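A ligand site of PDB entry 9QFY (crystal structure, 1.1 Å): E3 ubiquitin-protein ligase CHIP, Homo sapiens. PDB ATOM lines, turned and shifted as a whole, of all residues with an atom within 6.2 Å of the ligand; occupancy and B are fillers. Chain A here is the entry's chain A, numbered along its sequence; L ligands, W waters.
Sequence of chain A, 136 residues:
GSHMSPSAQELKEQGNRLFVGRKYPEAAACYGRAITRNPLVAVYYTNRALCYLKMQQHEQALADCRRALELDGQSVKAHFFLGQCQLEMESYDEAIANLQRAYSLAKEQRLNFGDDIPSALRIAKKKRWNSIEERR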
ATOM      1  N   GLY A  15      30.816   7.722  -4.975  1.00  0.00           N
ATOM      2  CA  GLY A  15      29.531   7.441  -4.334  1.00  0.00           C
ATOM      3  C   GLY A  15      28.913   6.172  -4.854  1.00  0.00           C
ATOM      4  O   GLY A  15      28.410   5.347  -4.082  1.00  0.00           O
ATOM      5  N   ASN A  16      28.968   5.956  -6.173  1.00  0.00           N
ATOM      6  CA  ASN A  16      28.440   4.734  -6.771  1.00  0.00           C
ATOM      7  C   ASN A  16      29.170   3.504  -6.240  1.00  0.00           C
ATOM      8  O   ASN A  16      28.533   2.493  -5.949  1.00  0.00           O
ATOM      9  CB  ASN A  16      28.551   4.795  -8.291  1.00  0.00           C
ATOM     10  CG  ASN A  16      27.547   5.719  -8.942  1.00  0.00           C
ATOM     11  OD1 ASN A  16      26.841   6.509  -8.306  1.00  0.00           O
ATOM     12  ND2 ASN A  16      27.452   5.631 -10.265  1.00  0.00           N
ATOM     13  N   ARG A  17      30.483   3.595  -6.100  1.00  0.00           N
ATOM     14  CA  ARG A  17      31.284   2.486  -5.597  1.00  0.00           C
ATOM     15  C   ARG A  17      30.969   2.210  -4.126  1.00  0.00           C
ATOM     16  O   ARG A  17      30.842   1.055  -3.707  1.00  0.00           O
ATOM     17  CB  ARG A  17      32.771   2.819  -5.805  1.00  0.00           C
ATOM     18  CG  ARG A  17      33.728   1.753  -5.303  1.00  0.00           C
ATOM     19  CD  ARG A  17      34.276   2.090  -3.926  1.00  0.00           C
ATOM     20  NE  ARG A  17      35.131   3.271  -3.981  1.00  0.00           N
ATOM     21  CZ  ARG A  17      35.703   3.842  -2.931  1.00  0.00           C
ATOM     22  NH1 ARG A  17      35.523   3.338  -1.702  1.00  0.00           N
ATOM     23  NH2 ARG A  17      36.463   4.913  -3.077  1.00  0.00           N
ATOM     24  N   PHE A  19      28.129   2.879  -2.658  1.00  0.00           N
ATOM     25  CA  PHE A  19      26.781   2.317  -2.646  1.00  0.00           C
ATOM     26  C   PHE A  19      26.828   0.822  -2.929  1.00  0.00           C
ATOM     27  O   PHE A  19      26.156   0.058  -2.233  1.00  0.00           O
ATOM     28  CB  PHE A  19      25.923   3.021  -3.697  1.00  0.00           C
ATOM     29  CG  PHE A  19      24.505   2.522  -3.661  1.00  0.00           C
ATOM     30  CD1 PHE A  19      23.584   3.076  -2.794  1.00  0.00           C
ATOM     31  CD2 PHE A  19      24.094   1.441  -4.442  1.00  0.00           C
ATOM     32  CE1 PHE A  19      22.279   2.600  -2.729  1.00  0.00           C
ATOM     33  CE2 PHE A  19      22.801   0.946  -4.348  1.00  0.00           C
ATOM     34  CZ  PHE A  19      21.916   1.519  -3.483  1.00  0.00           C
ATOM     35  N   VAL A  20      27.644   0.378  -3.894  1.00  0.00           N
ATOM     36  CA  VAL A  20      27.822  -1.053  -4.172  1.00  0.00           C
ATOM     37  C   VAL A  20      28.360  -1.779  -2.917  1.00  0.00           C
ATOM     38  O   VAL A  20      27.972  -2.903  -2.643  1.00  0.00           O
ATOM     39  CB  VAL A  20      28.730  -1.270  -5.401  1.00  0.00           C
ATOM     40  CG1 VAL A  20      29.140  -2.734  -5.538  1.00  0.00           C
ATOM     41  CG2 VAL A  20      28.021  -0.803  -6.667  1.00  0.00           C
ATOM     42  N   TYR A  31      27.841  12.190  -2.942  1.00  0.00           N
ATOM     43  CA  TYR A  31      26.932  12.893  -3.857  1.00  0.00           C
ATOM     44  C   TYR A  31      26.745  14.337  -3.450  1.00  0.00           C
ATOM     45  O   TYR A  31      26.673  15.186  -4.314  1.00  0.00           O
ATOM     46  CB  TYR A  31      25.594  12.173  -3.976  1.00  0.00           C
ATOM     47  CG  TYR A  31      25.713  10.760  -4.483  1.00  0.00           C
ATOM     48  CD1 TYR A  31      26.390  10.462  -5.656  1.00  0.00           C
ATOM     49  CD2 TYR A  31      25.125   9.713  -3.796  1.00  0.00           C
ATOM     50  CE1 TYR A  31      26.505   9.150  -6.112  1.00  0.00           C
ATOM     51  CE2 TYR A  31      25.225   8.409  -4.241  1.00  0.00           C
ATOM     52  CZ  TYR A  31      25.940   8.127  -5.392  1.00  0.00           C
ATOM     53  OH  TYR A  31      25.989   6.829  -5.838  1.00  0.00           O
ATOM     54  N   VAL A  43      21.454  13.208 -11.892  1.00  0.00           N
ATOM     55  CA  VAL A  43      21.858  11.879 -11.386  1.00  0.00           C
ATOM     56  C   VAL A  43      22.482  11.955  -9.988  1.00  0.00           C
ATOM     57  O   VAL A  43      22.381  10.975  -9.232  1.00  0.00           O
ATOM     58  CB  VAL A  43      22.750  11.103 -12.391  1.00  0.00           C
ATOM     59  CG1 VAL A  43      24.173  11.626 -12.456  1.00  0.00           C
ATOM     60  CG2 VAL A  43      22.699   9.607 -12.135  1.00  0.00           C
ATOM     61  N   THR A  46      19.339  11.718  -7.915  1.00  0.00           N
ATOM     62  CA  THR A  46      18.674  10.402  -7.959  1.00  0.00           C
ATOM     63  C   THR A  46      19.463   9.383  -7.165  1.00  0.00           C
ATOM     64  O   THR A  46      18.893   8.583  -6.430  1.00  0.00           O
ATOM     65  CB  THR A  46      18.475   9.909  -9.388  1.00  0.00           C
ATOM     66  OG1 THR A  46      19.705   9.665 -10.072  1.00  0.00           O
ATOM     67  CG2 THR A  46      17.614  10.812 -10.179  1.00  0.00           C
ATOM     68  N   ASN A  47      20.796   9.416  -7.309  1.00  0.00           N
ATOM     69  CA  ASN A  47      21.610   8.405  -6.618  1.00  0.00           C
ATOM     70  C   ASN A  47      21.574   8.639  -5.118  1.00  0.00           C
ATOM     71  O   ASN A  47      21.501   7.664  -4.345  1.00  0.00           O
ATOM     72  CB  ASN A  47      23.002   8.345  -7.211  1.00  0.00           C
ATOM     73  CG  ASN A  47      23.014   7.894  -8.658  1.00  0.00           C
ATOM     74  OD1 ASN A  47      21.975   7.728  -9.314  1.00  0.00           O
ATOM     75  ND2 ASN A  47      24.214   7.676  -9.197  1.00  0.00           N
ATOM     76  N   ARG A  48      21.618   9.910  -4.690  1.00  0.00           N
ATOM     77  CA  ARG A  48      21.526  10.197  -3.271  1.00  0.00           C
ATOM     78  C   ARG A  48      20.156   9.812  -2.728  1.00  0.00           C
ATOM     79  O   ARG A  48      20.074   9.311  -1.607  1.00  0.00           O
ATOM     80  CB  ARG A  48      21.864  11.661  -2.969  1.00  0.00           C
ATOM     81  CG  ARG A  48      22.032  11.865  -1.479  1.00  0.00           C
ATOM     82  CD  ARG A  48      22.558  13.228  -1.101  1.00  0.00           C
ATOM     83  NE  ARG A  48      21.604  14.271  -1.470  1.00  0.00           N
ATOM     84  CZ  ARG A  48      21.792  15.565  -1.269  1.00  0.00           C
ATOM     85  NH1 ARG A  48      22.915  15.988  -0.687  1.00  0.00           N
ATOM     86  NH2 ARG A  48      20.890  16.451  -1.673  1.00  0.00           N
ATOM     87  N   LEU A  50      18.331   7.251  -3.507  1.00  0.00           N
ATOM     88  CA  LEU A  50      18.306   5.821  -3.172  1.00  0.00           C
ATOM     89  C   LEU A  50      19.094   5.562  -1.877  1.00  0.00           C
ATOM     90  O   LEU A  50      18.685   4.740  -1.049  1.00  0.00           O
ATOM     91  CB  LEU A  50      18.840   4.982  -4.313  1.00  0.00           C
ATOM     92  CG  LEU A  50      18.752   3.472  -4.117  1.00  0.00           C
ATOM     93  CD1 LEU A  50      17.323   3.005  -3.802  1.00  0.00           C
ATOM     94  CD2 LEU A  50      19.266   2.761  -5.343  1.00  0.00           C
ATOM     95  N   CYS A  51      20.191   6.285  -1.647  1.00  0.00           N
ATOM     96  CA  CYS A  51      20.915   6.190  -0.357  1.00  0.00           C
ATOM     97  C   CYS A  51      19.996   6.543   0.793  1.00  0.00           C
ATOM     98  O   CYS A  51      19.925   5.809   1.784  1.00  0.00           O
ATOM     99  CB  CYS A  51      22.111   7.134  -0.360  1.00  0.00           C
ATOM    100  SG  CYS A  51      23.426   6.697  -1.510  1.00  0.00           S
ATOM    101  N   VAL A  76      14.160   7.967 -15.597  1.00  0.00           N
ATOM    102  CA  VAL A  76      13.589   6.683 -15.178  1.00  0.00           C
ATOM    103  C   VAL A  76      13.883   6.453 -13.677  1.00  0.00           C
ATOM    104  O   VAL A  76      12.969   6.155 -12.896  1.00  0.00           O
ATOM    105  CB  VAL A  76      14.145   5.519 -16.026  1.00  0.00           C
ATOM    106  CG1 VAL A  76      13.750   4.163 -15.438  1.00  0.00           C
ATOM    107  CG2 VAL A  76      13.699   5.632 -17.466  1.00  0.00           C
ATOM    108  N   LYS A  77      15.138   6.645 -13.262  1.00  0.00           N
ATOM    109  CA  LYS A  77      15.514   6.453 -11.844  1.00  0.00           C
ATOM    110  C   LYS A  77      14.710   7.339 -10.928  1.00  0.00           C
ATOM    111  O   LYS A  77      14.278   6.841  -9.888  1.00  0.00           O
ATOM    112  CB  LYS A  77      16.986   6.777 -11.598  1.00  0.00           C
ATOM    113  CG  LYS A  77      17.996   5.729 -11.935  1.00  0.00           C
ATOM    114  CD  LYS A  77      19.348   6.302 -11.518  1.00  0.00           C
ATOM    115  CE  LYS A  77      20.443   5.315 -11.669  1.00  0.00           C
ATOM    116  NZ  LYS A  77      21.728   6.035 -11.661  1.00  0.00           N
ATOM    117  N   ALA A  78      14.525   8.629 -11.247  1.00  0.00           N
ATOM    118  CA  ALA A  78      13.779   9.485 -10.323  1.00  0.00           C
ATOM    119  C   ALA A  78      12.354   8.994 -10.097  1.00  0.00           C
ATOM    120  O   ALA A  78      11.887   8.957  -8.962  1.00  0.00           O
ATOM    121  CB  ALA A  78      13.801  10.919 -10.779  1.00  0.00           C
ATOM    122  N   PHE A  80      11.251   5.860 -10.602  1.00  0.00           N
ATOM    123  CA  PHE A  80      11.290   4.545  -9.982  1.00  0.00           C
ATOM    124  C   PHE A  80      11.544   4.690  -8.478  1.00  0.00           C
ATOM    125  O   PHE A  80      10.864   4.057  -7.666  1.00  0.00           O
ATOM    126  CB  PHE A  80      12.361   3.675 -10.646  1.00  0.00           C
ATOM    127  CG  PHE A  80      12.329   2.236 -10.183  1.00  0.00           C
ATOM    128  CD1 PHE A  80      11.331   1.372 -10.618  1.00  0.00           C
ATOM    129  CD2 PHE A  80      13.270   1.759  -9.280  1.00  0.00           C
ATOM    130  CE1 PHE A  80      11.318   0.047 -10.194  1.00  0.00           C
ATOM    131  CE2 PHE A  80      13.234   0.429  -8.864  1.00  0.00           C
ATOM    132  CZ  PHE A  80      12.246  -0.408  -9.306  1.00  0.00           C
ATOM    133  N   PHE A  81      12.548   5.485  -8.096  1.00  0.00           N
ATOM    134  CA  PHE A  81      12.883   5.685  -6.689  1.00  0.00           C
ATOM    135  C   PHE A  81      11.768   6.422  -5.967  1.00  0.00           C
ATOM    136  O   PHE A  81      11.458   6.084  -4.819  1.00  0.00           O
ATOM    137  CB  PHE A  81      14.223   6.389  -6.498  1.00  0.00           C
ATOM    138  CG  PHE A  81      15.432   5.689  -7.078  1.00  0.00           C
ATOM    139  CD1 PHE A  81      15.410   4.333  -7.337  1.00  0.00           C
ATOM    140  CD2 PHE A  81      16.594   6.402  -7.350  1.00  0.00           C
ATOM    141  CE1 PHE A  81      16.524   3.699  -7.874  1.00  0.00           C
ATOM    142  CE2 PHE A  81      17.688   5.771  -7.898  1.00  0.00           C
ATOM    143  CZ  PHE A  81      17.657   4.429  -8.162  1.00  0.00           C
ATOM    144  N   ALA A 102       7.850   5.158 -14.729  1.00  0.00           N
ATOM    145  CA  ALA A 102       9.209   4.656 -14.927  1.00  0.00           C
ATOM    146  C   ALA A 102       9.197   3.565 -16.007  1.00  0.00           C
ATOM    147  O   ALA A 102      10.077   3.555 -16.847  1.00  0.00           O
ATOM    148  CB  ALA A 102       9.755   4.072 -13.616  1.00  0.00           C
ATOM    149  N   ALA A 106      11.284   3.935 -19.378  1.00  0.00           N
ATOM    150  CA  ALA A 106      12.330   2.941 -19.667  1.00  0.00           C
ATOM    151  C   ALA A 106      12.129   2.293 -21.020  1.00  0.00           C
ATOM    152  O   ALA A 106      13.107   2.042 -21.733  1.00  0.00           O
ATOM    153  CB  ALA A 106      12.370   1.887 -18.581  1.00  0.00           C
ATOM    154  N   PHE A 113      15.845  -3.320 -17.509  1.00  0.00           N
ATOM    155  CA  PHE A 113      15.910  -3.714 -16.112  1.00  0.00           C
ATOM    156  C   PHE A 113      15.222  -5.070 -15.917  1.00  0.00           C
ATOM    157  O   PHE A 113      14.704  -5.322 -14.842  1.00  0.00           O
ATOM    158  CB  PHE A 113      15.229  -2.661 -15.225  1.00  0.00           C
ATOM    159  CG  PHE A 113      15.931  -1.324 -15.219  1.00  0.00           C
ATOM    160  CD1 PHE A 113      17.088  -1.137 -14.488  1.00  0.00           C
ATOM    161  CD2 PHE A 113      15.443  -0.265 -15.959  1.00  0.00           C
ATOM    162  CE1 PHE A 113      17.733   0.090 -14.479  1.00  0.00           C
ATOM    163  CE2 PHE A 113      16.104   0.950 -15.974  1.00  0.00           C
ATOM    164  CZ  PHE A 113      17.233   1.131 -15.223  1.00  0.00           C
ATOM    165  N   ASP A 116      12.060  -6.055 -13.518  1.00  0.00           N
ATOM    166  CA  ASP A 116      12.022  -5.317 -12.265  1.00  0.00           C
ATOM    167  C   ASP A 116      10.857  -4.374 -12.124  1.00  0.00           C
ATOM    168  O   ASP A 116      10.263  -4.329 -11.058  1.00  0.00           O
ATOM    169  CB  ASP A 116      13.330  -4.535 -12.027  1.00  0.00           C
ATOM    170  CG  ASP A 116      14.563  -5.379 -11.774  1.00  0.00           C
ATOM    171  OD1 ASP A 116      14.432  -6.627 -11.721  1.00  0.00           O
ATOM    172  OD2 ASP A 116      15.662  -4.788 -11.631  1.00  0.00           O
ATOM    173  N   ILE A 117      10.543  -3.589 -13.184  1.00  0.00           N
ATOM    174  CA  ILE A 117       9.471  -2.614 -13.049  1.00  0.00           C
ATOM    175  C   ILE A 117       8.100  -3.282 -12.971  1.00  0.00           C
ATOM    176  O   ILE A 117       7.358  -2.990 -12.034  1.00  0.00           O
ATOM    177  CB  ILE A 117       9.528  -1.437 -14.033  1.00  0.00           C
ATOM    178  CG1 ILE A 117      10.929  -0.809 -14.057  1.00  0.00           C
ATOM    179  CG2 ILE A 117       8.487  -0.409 -13.649  1.00  0.00           C
ATOM    180  CD1 ILE A 117      11.182   0.145 -15.218  1.00  0.00           C
HETATM  181  C1  LIG L   1      22.737   4.846  -5.878  1.00  0.00           C
HETATM  182  C2  LIG L   1      22.185   2.451  -8.150  1.00  0.00           C
HETATM  183  C3  LIG L   1      21.119   1.857  -9.067  1.00  0.00           C
HETATM  184  C4  LIG L   1      20.716   0.492  -8.523  1.00  0.00           C
HETATM  185  C5  LIG L   1      18.460  -0.350  -8.880  1.00  0.00           C
HETATM  186  C6  LIG L   1      17.397  -0.818  -9.813  1.00  0.00           C
HETATM  187  C7  LIG L   1      16.926  -2.111  -9.885  1.00  0.00           C
HETATM  188  C8  LIG L   1      15.620  -0.926 -11.245  1.00  0.00           C
HETATM  189  C9  LIG L   1      16.537  -0.029 -10.666  1.00  0.00           C
HETATM  190  C10 LIG L   1      16.459   1.312 -11.024  1.00  0.00           C
HETATM  191  C11 LIG L   1      15.498   1.756 -11.913  1.00  0.00           C
HETATM  192  C12 LIG L   1      14.605   0.878 -12.472  1.00  0.00           C
HETATM  193  C13 LIG L   1      14.676  -0.458 -12.146  1.00  0.00           C
HETATM  194  F1  LIG L   1      17.331   2.204 -10.524  1.00  0.00           F
HETATM  195  F2  LIG L   1      15.459   3.050 -12.275  1.00  0.00           F
HETATM  196  F3  LIG L   1      13.674   1.319 -13.334  1.00  0.00           F
HETATM  197  F4  LIG L   1      13.790  -1.323 -12.686  1.00  0.00           F
HETATM  198  N1  LIG L   1      15.914  -2.188 -10.795  1.00  0.00           N
HETATM  199  O1  LIG L   1      18.196  -0.212  -7.682  1.00  0.00           O
HETATM  200  N2  LIG L   1      19.676  -0.094  -9.373  1.00  0.00           N
HETATM  201  C14 LIG L   1      20.099  -0.335 -10.758  1.00  0.00           C
HETATM  202  C15 LIG L   1      20.578   0.969 -11.394  1.00  0.00           C
HETATM  203  C16 LIG L   1      21.609   1.675 -10.514  1.00  0.00           C
HETATM  204  S1  LIG L   1      22.353   4.204  -8.393  1.00  0.00           S
HETATM  205  O2  LIG L   1      21.079   4.818  -8.196  1.00  0.00           O
HETATM  206  O3  LIG L   1      23.049   4.407  -9.632  1.00  0.00           O
HETATM  207  N3  LIG L   1      23.323   4.715  -7.209  1.00  0.00           N
HETATM  208  C17 LIG L   1      24.679   4.153  -7.218  1.00  0.00           C
HETATM  209  O   HOH W   1      19.804  -1.213  -5.494  1.00  0.00           O
HETATM  210  O   HOH W   2      23.828   4.171 -12.677  1.00  0.00           O
HETATM  211  O   HOH W   3      26.545   1.650  -8.197  1.00  0.00           O
HETATM  212  O   HOH W   4      15.843   0.052  -5.982  1.00  0.00           O
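OD1 of Asn 47 sits at hydrogen-bond distance from NZ of Lys 77 (2.9 Å).
The side-chain amide nitrogen of Asn 47 sits at hydrogen-bond distance from the side-chain amide oxygen of Asn 16 (3.0 Å).
OD1 of Asn 47 is in hydrogen-bond range of OG1 of Thr 46.
O of Asn 47 is in hydrogen-bond range of SG of Cys 51.
OD1 of Asn 47 lies close to O of Val 43, 3.3 Å away.
The side-chain hydroxyl (OH) of Tyr 31 lies within hydrogen-bond range of the side-chain amide oxygen (OD1) of Asn 16, 2.6 Å away.
The side-chain hydroxyl (OH) of Tyr 31 sits close to the backbone carbonyl oxygen (O) of Gly 15, at 3.3 Å.
A nitrogen (N1) of the ligand sits at hydrogen-bond distance from the side-chain carboxylate of Asp 116 (2.7 Å).
The side-chain amino group (NZ) of Lys 77 is in hydrogen-bond range of an oxygen (O3) of the ligand (2.9 Å).
The side-chain amide oxygen (OD1) of Asn 47 sits close to an oxygen (O2) of the ligand (3.2 Å).
Water W2 bridges the side-chain amino group of Lys 77 (3.0 Å) and an oxygen (O3) of the ligand (3.2 Å).
Residues that only touch the ligand: Phe 81 (3.1 Å), Phe 113 (3.2 Å), Ile 117 (3.2 Å), Tyr 31 (3.3 Å), Asn 16 (3.4 Å), Phe 80 (3.4 Å), Val 76 (3.5 Å), Phe 19 (3.7 Å) and Leu 50 (3.9 Å).
Of the 22 residues printed, 12 come within 4 Å of the ligand.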
